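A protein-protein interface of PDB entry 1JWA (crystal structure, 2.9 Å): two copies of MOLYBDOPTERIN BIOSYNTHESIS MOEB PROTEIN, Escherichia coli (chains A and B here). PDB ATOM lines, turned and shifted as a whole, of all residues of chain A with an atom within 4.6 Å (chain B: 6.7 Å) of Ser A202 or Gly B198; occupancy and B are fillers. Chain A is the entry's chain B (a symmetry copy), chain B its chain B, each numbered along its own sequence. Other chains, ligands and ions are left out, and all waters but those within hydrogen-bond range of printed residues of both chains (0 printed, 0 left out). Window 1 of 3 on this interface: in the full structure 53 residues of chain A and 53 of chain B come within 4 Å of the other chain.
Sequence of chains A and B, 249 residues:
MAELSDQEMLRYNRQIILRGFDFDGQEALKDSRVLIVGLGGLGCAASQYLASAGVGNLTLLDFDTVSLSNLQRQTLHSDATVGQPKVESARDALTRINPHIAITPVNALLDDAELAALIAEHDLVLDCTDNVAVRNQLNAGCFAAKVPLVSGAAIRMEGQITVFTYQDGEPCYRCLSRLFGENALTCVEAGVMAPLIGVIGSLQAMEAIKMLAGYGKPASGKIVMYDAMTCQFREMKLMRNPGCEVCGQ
The backbone carbonyl oxygen of Gly B198 lies within hydrogen-bond range of the side-chain hydroxyl of Ser B202. The backbone carbonyl oxygen (O) of Gly A198 lies within hydrogen-bond range of the side-chain hydroxyl (OG) of Ser A202 (3.2 Å).
Tyr A49 touches Gly B198, and with the chains exchanged Gly A198 touches Tyr B49. Gly A198 touches Ser B202, and with the chains exchanged Ser A202 touches Gly B198. Val A199 touches Ser B202, and with the chains exchanged Ser A202 touches Val B199. Val A199 touches Leu B203, and with the chains exchanged Leu A203 touches Val B199. 7 positions are printed for both chains. Of the 15 pairs that touch across the chains among the printed residues, 8 have their exchanged pair printed and touching as well.
Printed residues of chain A that touch a printed residue of chain B: Tyr A49, Gly A198, Val A199, Ser A202, Leu A203 and Met A206. Hydrophobic or aromatic side chains of chain A that line the printed part of chain B: Tyr A49, Val A199, Leu A203 and Met A206. Of the 17 printed residues of chain B, 10 touch a printed residue of chain A. Hydrophobic or aromatic side chains of chain B that line the printed part of chain A: Ala B45, Tyr B49, Met B193, Pro B195, Leu B196, Val B199, Leu B203 and Tyr B226. Along chain B the printed residues that touch a printed residue of chain A span positions 45 to 226.
Of the printed residues of chain B, Tyr A49 touches Ala B45 (3.7 Å) and Gly B198 (3.6 Å). Ser A202 touches three residues of chain B. Printed residues of chain A within 4 Å of Ala B45: Tyr A49. Of the printed residues of chain A, Met B193 touches Met A206. Of chain A, only Tyr A49 and Ser A202 come within 4 Å of Gly B198. Of the printed residues of chain A, Val B199 touches Ser A202 (3.5 Å) and Leu A203 (3.9 Å). Of the printed residues of chain A, Leu B203 touches Val A199 (3.9 Å). The nearest printed residue of chain A that does not touch Met B193 is Ala A205 (6.7 Å).
Among the printed residues, merely in contact across the chains: Gly A198 with Ser B202 (3.3 Å), Ser A202 with Gly B198 (3.3 Å), Leu A203 with Tyr B226 (3.5 Å), Ser A202 with Val B199 (3.5 Å), Val A199 with Ser B202 (3.5 Å), Met A206 with Leu B196 (3.5 Å), Ser A202 with Pro B195 (3.6 Å), Gly A198 with Tyr B49 (3.6 Å), Tyr A49 with Gly B198 (3.6 Å), Tyr A49 with Ala B45 (3.7 Å), Met A206 with Tyr B226 (3.7 Å), Met A206 with Pro B195 (3.7 Å), Met A206 with Met B193 (3.7 Å), Leu A203 with Val B199 (3.9 Å) and Val A199 with Leu B203 (3.9 Å).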
ATOM      1  N   TYR A  49     -35.038 -18.422   0.493  1.00  0.00           N
ATOM      2  CA  TYR A  49     -34.589 -19.742   0.939  1.00  0.00           C
ATOM      3  C   TYR A  49     -35.359 -20.224   2.141  1.00  0.00           C
ATOM      4  O   TYR A  49     -35.348 -21.390   2.478  1.00  0.00           O
ATOM      5  CB  TYR A  49     -33.102 -19.723   1.272  1.00  0.00           C
ATOM      6  CG  TYR A  49     -32.222 -19.514   0.064  1.00  0.00           C
ATOM      7  CD1 TYR A  49     -31.467 -18.354  -0.091  1.00  0.00           C
ATOM      8  CD2 TYR A  49     -32.164 -20.466  -0.930  1.00  0.00           C
ATOM      9  CE1 TYR A  49     -30.684 -18.162  -1.203  1.00  0.00           C
ATOM     10  CE2 TYR A  49     -31.379 -20.294  -2.030  1.00  0.00           C
ATOM     11  CZ  TYR A  49     -30.633 -19.132  -2.165  1.00  0.00           C
ATOM     12  OH  TYR A  49     -29.840 -18.931  -3.268  1.00  0.00           O
ATOM     13  N   GLY A 198     -26.547 -11.129  -0.573  1.00  0.00           N
ATOM     14  CA  GLY A 198     -26.853 -12.540  -0.753  1.00  0.00           C
ATOM     15  C   GLY A 198     -26.116 -13.447   0.225  1.00  0.00           C
ATOM     16  O   GLY A 198     -26.668 -14.404   0.780  1.00  0.00           O
ATOM     17  N   VAL A 199     -24.869 -13.101   0.464  1.00  0.00           N
ATOM     18  CA  VAL A 199     -24.059 -13.801   1.419  1.00  0.00           C
ATOM     19  C   VAL A 199     -24.719 -13.676   2.772  1.00  0.00           C
ATOM     20  O   VAL A 199     -24.996 -14.669   3.404  1.00  0.00           O
ATOM     21  CB  VAL A 199     -22.685 -13.153   1.539  1.00  0.00           C
ATOM     22  CG1 VAL A 199     -21.869 -13.855   2.577  1.00  0.00           C
ATOM     23  CG2 VAL A 199     -22.007 -13.171   0.224  1.00  0.00           C
ATOM     24  N   ILE A 200     -24.955 -12.449   3.211  1.00  0.00           N
ATOM     25  CA  ILE A 200     -25.505 -12.212   4.529  1.00  0.00           C
ATOM     26  C   ILE A 200     -26.930 -12.721   4.610  1.00  0.00           C
ATOM     27  O   ILE A 200     -27.340 -13.310   5.619  1.00  0.00           O
ATOM     28  CB  ILE A 200     -25.495 -10.698   4.855  1.00  0.00           C
ATOM     29  CG1 ILE A 200     -24.078 -10.207   5.071  1.00  0.00           C
ATOM     30  CG2 ILE A 200     -26.338 -10.382   6.115  1.00  0.00           C
ATOM     31  CD1 ILE A 200     -23.369 -10.842   6.294  1.00  0.00           C
ATOM     32  N   GLY A 201     -27.710 -12.465   3.570  1.00  0.00           N
ATOM     33  CA  GLY A 201     -29.086 -12.912   3.602  1.00  0.00           C
ATOM     34  C   GLY A 201     -29.234 -14.417   3.754  1.00  0.00           C
ATOM     35  O   GLY A 201     -30.000 -14.905   4.552  1.00  0.00           O
ATOM     36  N   SER A 202     -28.496 -15.174   2.966  1.00  0.00           N
ATOM     37  CA  SER A 202     -28.556 -16.621   3.069  1.00  0.00           C
ATOM     38  C   SER A 202     -28.005 -17.096   4.396  1.00  0.00           C
ATOM     39  O   SER A 202     -28.344 -18.177   4.838  1.00  0.00           O
ATOM     40  CB  SER A 202     -27.719 -17.250   1.973  1.00  0.00           C
ATOM     41  OG  SER A 202     -28.289 -17.129   0.732  1.00  0.00           O
ATOM     42  N   LEU A 203     -27.132 -16.313   5.032  1.00  0.00           N
ATOM     43  CA  LEU A 203     -26.621 -16.698   6.362  1.00  0.00           C
ATOM     44  C   LEU A 203     -27.799 -16.698   7.362  1.00  0.00           C
ATOM     45  O   LEU A 203     -28.029 -17.653   8.115  1.00  0.00           O
ATOM     46  CB  LEU A 203     -25.514 -15.765   6.844  1.00  0.00           C
ATOM     47  CG  LEU A 203     -24.110 -16.100   6.312  1.00  0.00           C
ATOM     48  CD1 LEU A 203     -23.019 -15.149   6.852  1.00  0.00           C
ATOM     49  CD2 LEU A 203     -23.735 -17.542   6.604  1.00  0.00           C
ATOM     50  N   GLN A 204     -28.560 -15.609   7.317  1.00  0.00           N
ATOM     51  CA  GLN A 204     -29.690 -15.458   8.174  1.00  0.00           C
ATOM     52  C   GLN A 204     -30.603 -16.671   7.994  1.00  0.00           C
ATOM     53  O   GLN A 204     -30.890 -17.397   8.946  1.00  0.00           O
ATOM     54  CB  GLN A 204     -30.423 -14.173   7.832  1.00  0.00           C
ATOM     55  CG  GLN A 204     -29.631 -12.910   8.064  1.00  0.00           C
ATOM     56  CD  GLN A 204     -30.499 -11.619   7.999  1.00  0.00           C
ATOM     57  OE1 GLN A 204     -30.530 -10.901   6.996  1.00  0.00           O
ATOM     58  NE2 GLN A 204     -31.130 -11.309   9.099  1.00  0.00           N
ATOM     59  N   ALA A 205     -31.072 -16.890   6.774  1.00  0.00           N
ATOM     60  CA  ALA A 205     -32.038 -17.983   6.495  1.00  0.00           C
ATOM     61  C   ALA A 205     -31.540 -19.329   7.030  1.00  0.00           C
ATOM     62  O   ALA A 205     -32.322 -20.169   7.412  1.00  0.00           O
ATOM     63  CB  ALA A 205     -32.324 -18.074   5.015  1.00  0.00           C
ATOM     64  N   MET A 206     -30.222 -19.505   7.077  1.00  0.00           N
ATOM     65  CA  MET A 206     -29.622 -20.723   7.602  1.00  0.00           C
ATOM     66  C   MET A 206     -29.832 -20.800   9.115  1.00  0.00           C
ATOM     67  O   MET A 206     -30.404 -21.730   9.666  1.00  0.00           O
ATOM     68  CB  MET A 206     -28.135 -20.681   7.311  1.00  0.00           C
ATOM     69  CG  MET A 206     -27.336 -21.890   7.809  1.00  0.00           C
ATOM     70  SD  MET A 206     -27.993 -23.413   7.334  1.00  0.00           S
ATOM     71  CE  MET A 206     -27.351 -23.675   5.732  1.00  0.00           C
ATOM     72  N   GLY B  41     -28.029 -26.114  -8.091  1.00  0.00           N
ATOM     73  CA  GLY B  41     -28.055 -25.442  -6.821  1.00  0.00           C
ATOM     74  C   GLY B  41     -27.225 -24.198  -6.759  1.00  0.00           C
ATOM     75  O   GLY B  41     -27.728 -23.092  -6.509  1.00  0.00           O
ATOM     76  N   LEU B  42     -25.939 -24.324  -7.039  1.00  0.00           N
ATOM     77  CA  LEU B  42     -25.065 -23.132  -7.042  1.00  0.00           C
ATOM     78  C   LEU B  42     -25.199 -22.283  -8.317  1.00  0.00           C
ATOM     79  O   LEU B  42     -25.335 -21.087  -8.278  1.00  0.00           O
ATOM     80  CB  LEU B  42     -23.621 -23.545  -6.868  1.00  0.00           C
ATOM     81  CG  LEU B  42     -23.221 -23.819  -5.430  1.00  0.00           C
ATOM     82  CD1 LEU B  42     -21.983 -24.678  -5.359  1.00  0.00           C
ATOM     83  CD2 LEU B  42     -22.969 -22.500  -4.694  1.00  0.00           C
ATOM     84  N   ALA B  45     -27.848 -19.844  -7.735  1.00  0.00           N
ATOM     85  CA  ALA B  45     -27.616 -18.801  -6.731  1.00  0.00           C
ATOM     86  C   ALA B  45     -26.728 -17.704  -7.233  1.00  0.00           C
ATOM     87  O   ALA B  45     -26.934 -16.527  -6.948  1.00  0.00           O
ATOM     88  CB  ALA B  45     -26.982 -19.434  -5.490  1.00  0.00           C
ATOM     89  N   ALA B  46     -25.686 -18.112  -7.937  1.00  0.00           N
ATOM     90  CA  ALA B  46     -24.679 -17.175  -8.393  1.00  0.00           C
ATOM     91  C   ALA B  46     -25.168 -16.382  -9.546  1.00  0.00           C
ATOM     92  O   ALA B  46     -24.877 -15.228  -9.623  1.00  0.00           O
ATOM     93  CB  ALA B  46     -23.368 -17.890  -8.745  1.00  0.00           C
ATOM     94  N   TYR B  49     -27.362 -13.014  -9.075  1.00  0.00           N
ATOM     95  CA  TYR B  49     -26.709 -11.765  -8.677  1.00  0.00           C
ATOM     96  C   TYR B  49     -25.711 -11.299  -9.705  1.00  0.00           C
ATOM     97  O   TYR B  49     -25.288 -10.161  -9.709  1.00  0.00           O
ATOM     98  CB  TYR B  49     -26.007 -11.928  -7.334  1.00  0.00           C
ATOM     99  CG  TYR B  49     -26.961 -12.132  -6.182  1.00  0.00           C
ATOM    100  CD1 TYR B  49     -27.010 -13.337  -5.488  1.00  0.00           C
ATOM    101  CD2 TYR B  49     -27.825 -11.127  -5.805  1.00  0.00           C
ATOM    102  CE1 TYR B  49     -27.894 -13.523  -4.453  1.00  0.00           C
ATOM    103  CE2 TYR B  49     -28.695 -11.294  -4.771  1.00  0.00           C
ATOM    104  CZ  TYR B  49     -28.728 -12.502  -4.090  1.00  0.00           C
ATOM    105  OH  TYR B  49     -29.602 -12.697  -3.049  1.00  0.00           O
ATOM    106  N   MET B 193     -28.858 -28.546   2.967  1.00  0.00           N
ATOM    107  CA  MET B 193     -29.732 -27.463   3.474  1.00  0.00           C
ATOM    108  C   MET B 193     -29.833 -26.324   2.430  1.00  0.00           C
ATOM    109  O   MET B 193     -28.846 -25.848   1.907  1.00  0.00           O
ATOM    110  CB  MET B 193     -29.165 -26.967   4.788  1.00  0.00           C
ATOM    111  CG  MET B 193     -30.109 -26.202   5.666  1.00  0.00           C
ATOM    112  SD  MET B 193     -31.621 -27.073   6.037  1.00  0.00           S
ATOM    113  CE  MET B 193     -30.977 -28.534   6.758  1.00  0.00           C
ATOM    114  N   ALA B 194     -31.035 -25.923   2.085  1.00  0.00           N
ATOM    115  CA  ALA B 194     -31.227 -24.916   1.036  1.00  0.00           C
ATOM    116  C   ALA B 194     -30.328 -23.639   1.123  1.00  0.00           C
ATOM    117  O   ALA B 194     -29.580 -23.324   0.192  1.00  0.00           O
ATOM    118  CB  ALA B 194     -32.718 -24.541   0.922  1.00  0.00           C
ATOM    119  N   PRO B 195     -30.375 -22.922   2.228  1.00  0.00           N
ATOM    120  CA  PRO B 195     -29.568 -21.720   2.337  1.00  0.00           C
ATOM    121  C   PRO B 195     -28.057 -21.902   2.173  1.00  0.00           C
ATOM    122  O   PRO B 195     -27.426 -20.918   1.930  1.00  0.00           O
ATOM    123  CB  PRO B 195     -29.924 -21.182   3.721  1.00  0.00           C
ATOM    124  CG  PRO B 195     -30.624 -22.236   4.426  1.00  0.00           C
ATOM    125  CD  PRO B 195     -31.165 -23.162   3.432  1.00  0.00           C
ATOM    126  N   LEU B 196     -27.491 -23.099   2.240  1.00  0.00           N
ATOM    127  CA  LEU B 196     -26.015 -23.274   2.102  1.00  0.00           C
ATOM    128  C   LEU B 196     -25.524 -22.991   0.693  1.00  0.00           C
ATOM    129  O   LEU B 196     -24.453 -22.469   0.441  1.00  0.00           O
ATOM    130  CB  LEU B 196     -25.608 -24.693   2.513  1.00  0.00           C
ATOM    131  CG  LEU B 196     -24.192 -25.178   2.216  1.00  0.00           C
ATOM    132  CD1 LEU B 196     -23.259 -24.865   3.347  1.00  0.00           C
ATOM    133  CD2 LEU B 196     -24.163 -26.669   1.938  1.00  0.00           C
ATOM    134  N   ILE B 197     -26.349 -23.333  -0.247  1.00  0.00           N
ATOM    135  CA  ILE B 197     -26.023 -23.153  -1.637  1.00  0.00           C
ATOM    136  C   ILE B 197     -26.046 -21.655  -1.888  1.00  0.00           C
ATOM    137  O   ILE B 197     -25.392 -21.200  -2.801  1.00  0.00           O
ATOM    138  CB  ILE B 197     -27.094 -23.932  -2.469  1.00  0.00           C
ATOM    139  CG1 ILE B 197     -26.421 -24.846  -3.415  1.00  0.00           C
ATOM    140  CG2 ILE B 197     -28.104 -23.040  -3.144  1.00  0.00           C
ATOM    141  CD1 ILE B 197     -26.434 -26.261  -2.914  1.00  0.00           C
ATOM    142  N   GLY B 198     -26.797 -20.897  -1.077  1.00  0.00           N
ATOM    143  CA  GLY B 198     -26.934 -19.457  -1.235  1.00  0.00           C
ATOM    144  C   GLY B 198     -25.729 -18.677  -0.727  1.00  0.00           C
ATOM    145  O   GLY B 198     -25.257 -17.714  -1.344  1.00  0.00           O
ATOM    146  N   VAL B 199     -25.206 -19.137   0.389  1.00  0.00           N
ATOM    147  CA  VAL B 199     -24.019 -18.568   0.962  1.00  0.00           C
ATOM    148  C   VAL B 199     -22.897 -18.723  -0.038  1.00  0.00           C
ATOM    149  O   VAL B 199     -22.279 -17.752  -0.408  1.00  0.00           O
ATOM    150  CB  VAL B 199     -23.603 -19.332   2.213  1.00  0.00           C
ATOM    151  CG1 VAL B 199     -22.336 -18.766   2.769  1.00  0.00           C
ATOM    152  CG2 VAL B 199     -24.693 -19.288   3.212  1.00  0.00           C
ATOM    153  N   ILE B 200     -22.636 -19.951  -0.457  1.00  0.00           N
ATOM    154  CA  ILE B 200     -21.529 -20.224  -1.348  1.00  0.00           C
ATOM    155  C   ILE B 200     -21.776 -19.606  -2.710  1.00  0.00           C
ATOM    156  O   ILE B 200     -20.862 -19.050  -3.333  1.00  0.00           O
ATOM    157  CB  ILE B 200     -21.336 -21.752  -1.520  1.00  0.00           C
ATOM    158  CG1 ILE B 200     -20.803 -22.370  -0.243  1.00  0.00           C
ATOM    159  CG2 ILE B 200     -20.366 -22.076  -2.682  1.00  0.00           C
ATOM    160  CD1 ILE B 200     -19.390 -21.873   0.158  1.00  0.00           C
ATOM    161  N   GLY B 201     -22.999 -19.732  -3.203  1.00  0.00           N
ATOM    162  CA  GLY B 201     -23.286 -19.177  -4.508  1.00  0.00           C
ATOM    163  C   GLY B 201     -23.055 -17.678  -4.596  1.00  0.00           C
ATOM    164  O   GLY B 201     -22.444 -17.180  -5.513  1.00  0.00           O
ATOM    165  N   SER B 202     -23.561 -16.936  -3.631  1.00  0.00           N
ATOM    166  CA  SER B 202     -23.359 -15.498  -3.625  1.00  0.00           C
ATOM    167  C   SER B 202     -21.901 -15.154  -3.414  1.00  0.00           C
ATOM    168  O   SER B 202     -21.474 -14.078  -3.788  1.00  0.00           O
ATOM    169  CB  SER B 202     -24.147 -14.872  -2.491  1.00  0.00           C
ATOM    170  OG  SER B 202     -25.498 -14.867  -2.721  1.00  0.00           O
ATOM    171  N   LEU B 203     -21.127 -16.044  -2.789  1.00  0.00           N
ATOM    172  CA  LEU B 203     -19.683 -15.786  -2.624  1.00  0.00           C
ATOM    173  C   LEU B 203     -19.025 -15.752  -4.021  1.00  0.00           C
ATOM    174  O   LEU B 203     -18.281 -14.831  -4.381  1.00  0.00           O
ATOM    175  CB  LEU B 203     -19.010 -16.835  -1.743  1.00  0.00           C
ATOM    176  CG  LEU B 203     -19.133 -16.584  -0.231  1.00  0.00           C
ATOM    177  CD1 LEU B 203     -18.410 -17.652   0.618  1.00  0.00           C
ATOM    178  CD2 LEU B 203     -18.637 -15.198   0.144  1.00  0.00           C
ATOM    179  N   TYR B 226     -16.642 -23.130   4.743  1.00  0.00           N
ATOM    180  CA  TYR B 226     -17.752 -22.629   5.574  1.00  0.00           C
ATOM    181  C   TYR B 226     -18.411 -23.791   6.200  1.00  0.00           C
ATOM    182  O   TYR B 226     -18.838 -24.673   5.481  1.00  0.00           O
ATOM    183  CB  TYR B 226     -18.772 -21.902   4.711  1.00  0.00           C
ATOM    184  CG  TYR B 226     -20.149 -21.665   5.311  1.00  0.00           C
ATOM    185  CD1 TYR B 226     -20.319 -21.093   6.546  1.00  0.00           C
ATOM    186  CD2 TYR B 226     -21.267 -21.939   4.598  1.00  0.00           C
ATOM    187  CE1 TYR B 226     -21.558 -20.847   7.052  1.00  0.00           C
ATOM    188  CE2 TYR B 226     -22.509 -21.717   5.111  1.00  0.00           C
ATOM    189  CZ  TYR B 226     -22.658 -21.166   6.317  1.00  0.00           C
ATOM    190  OH  TYR B 226     -23.949 -20.985   6.769  1.00  0.00           O
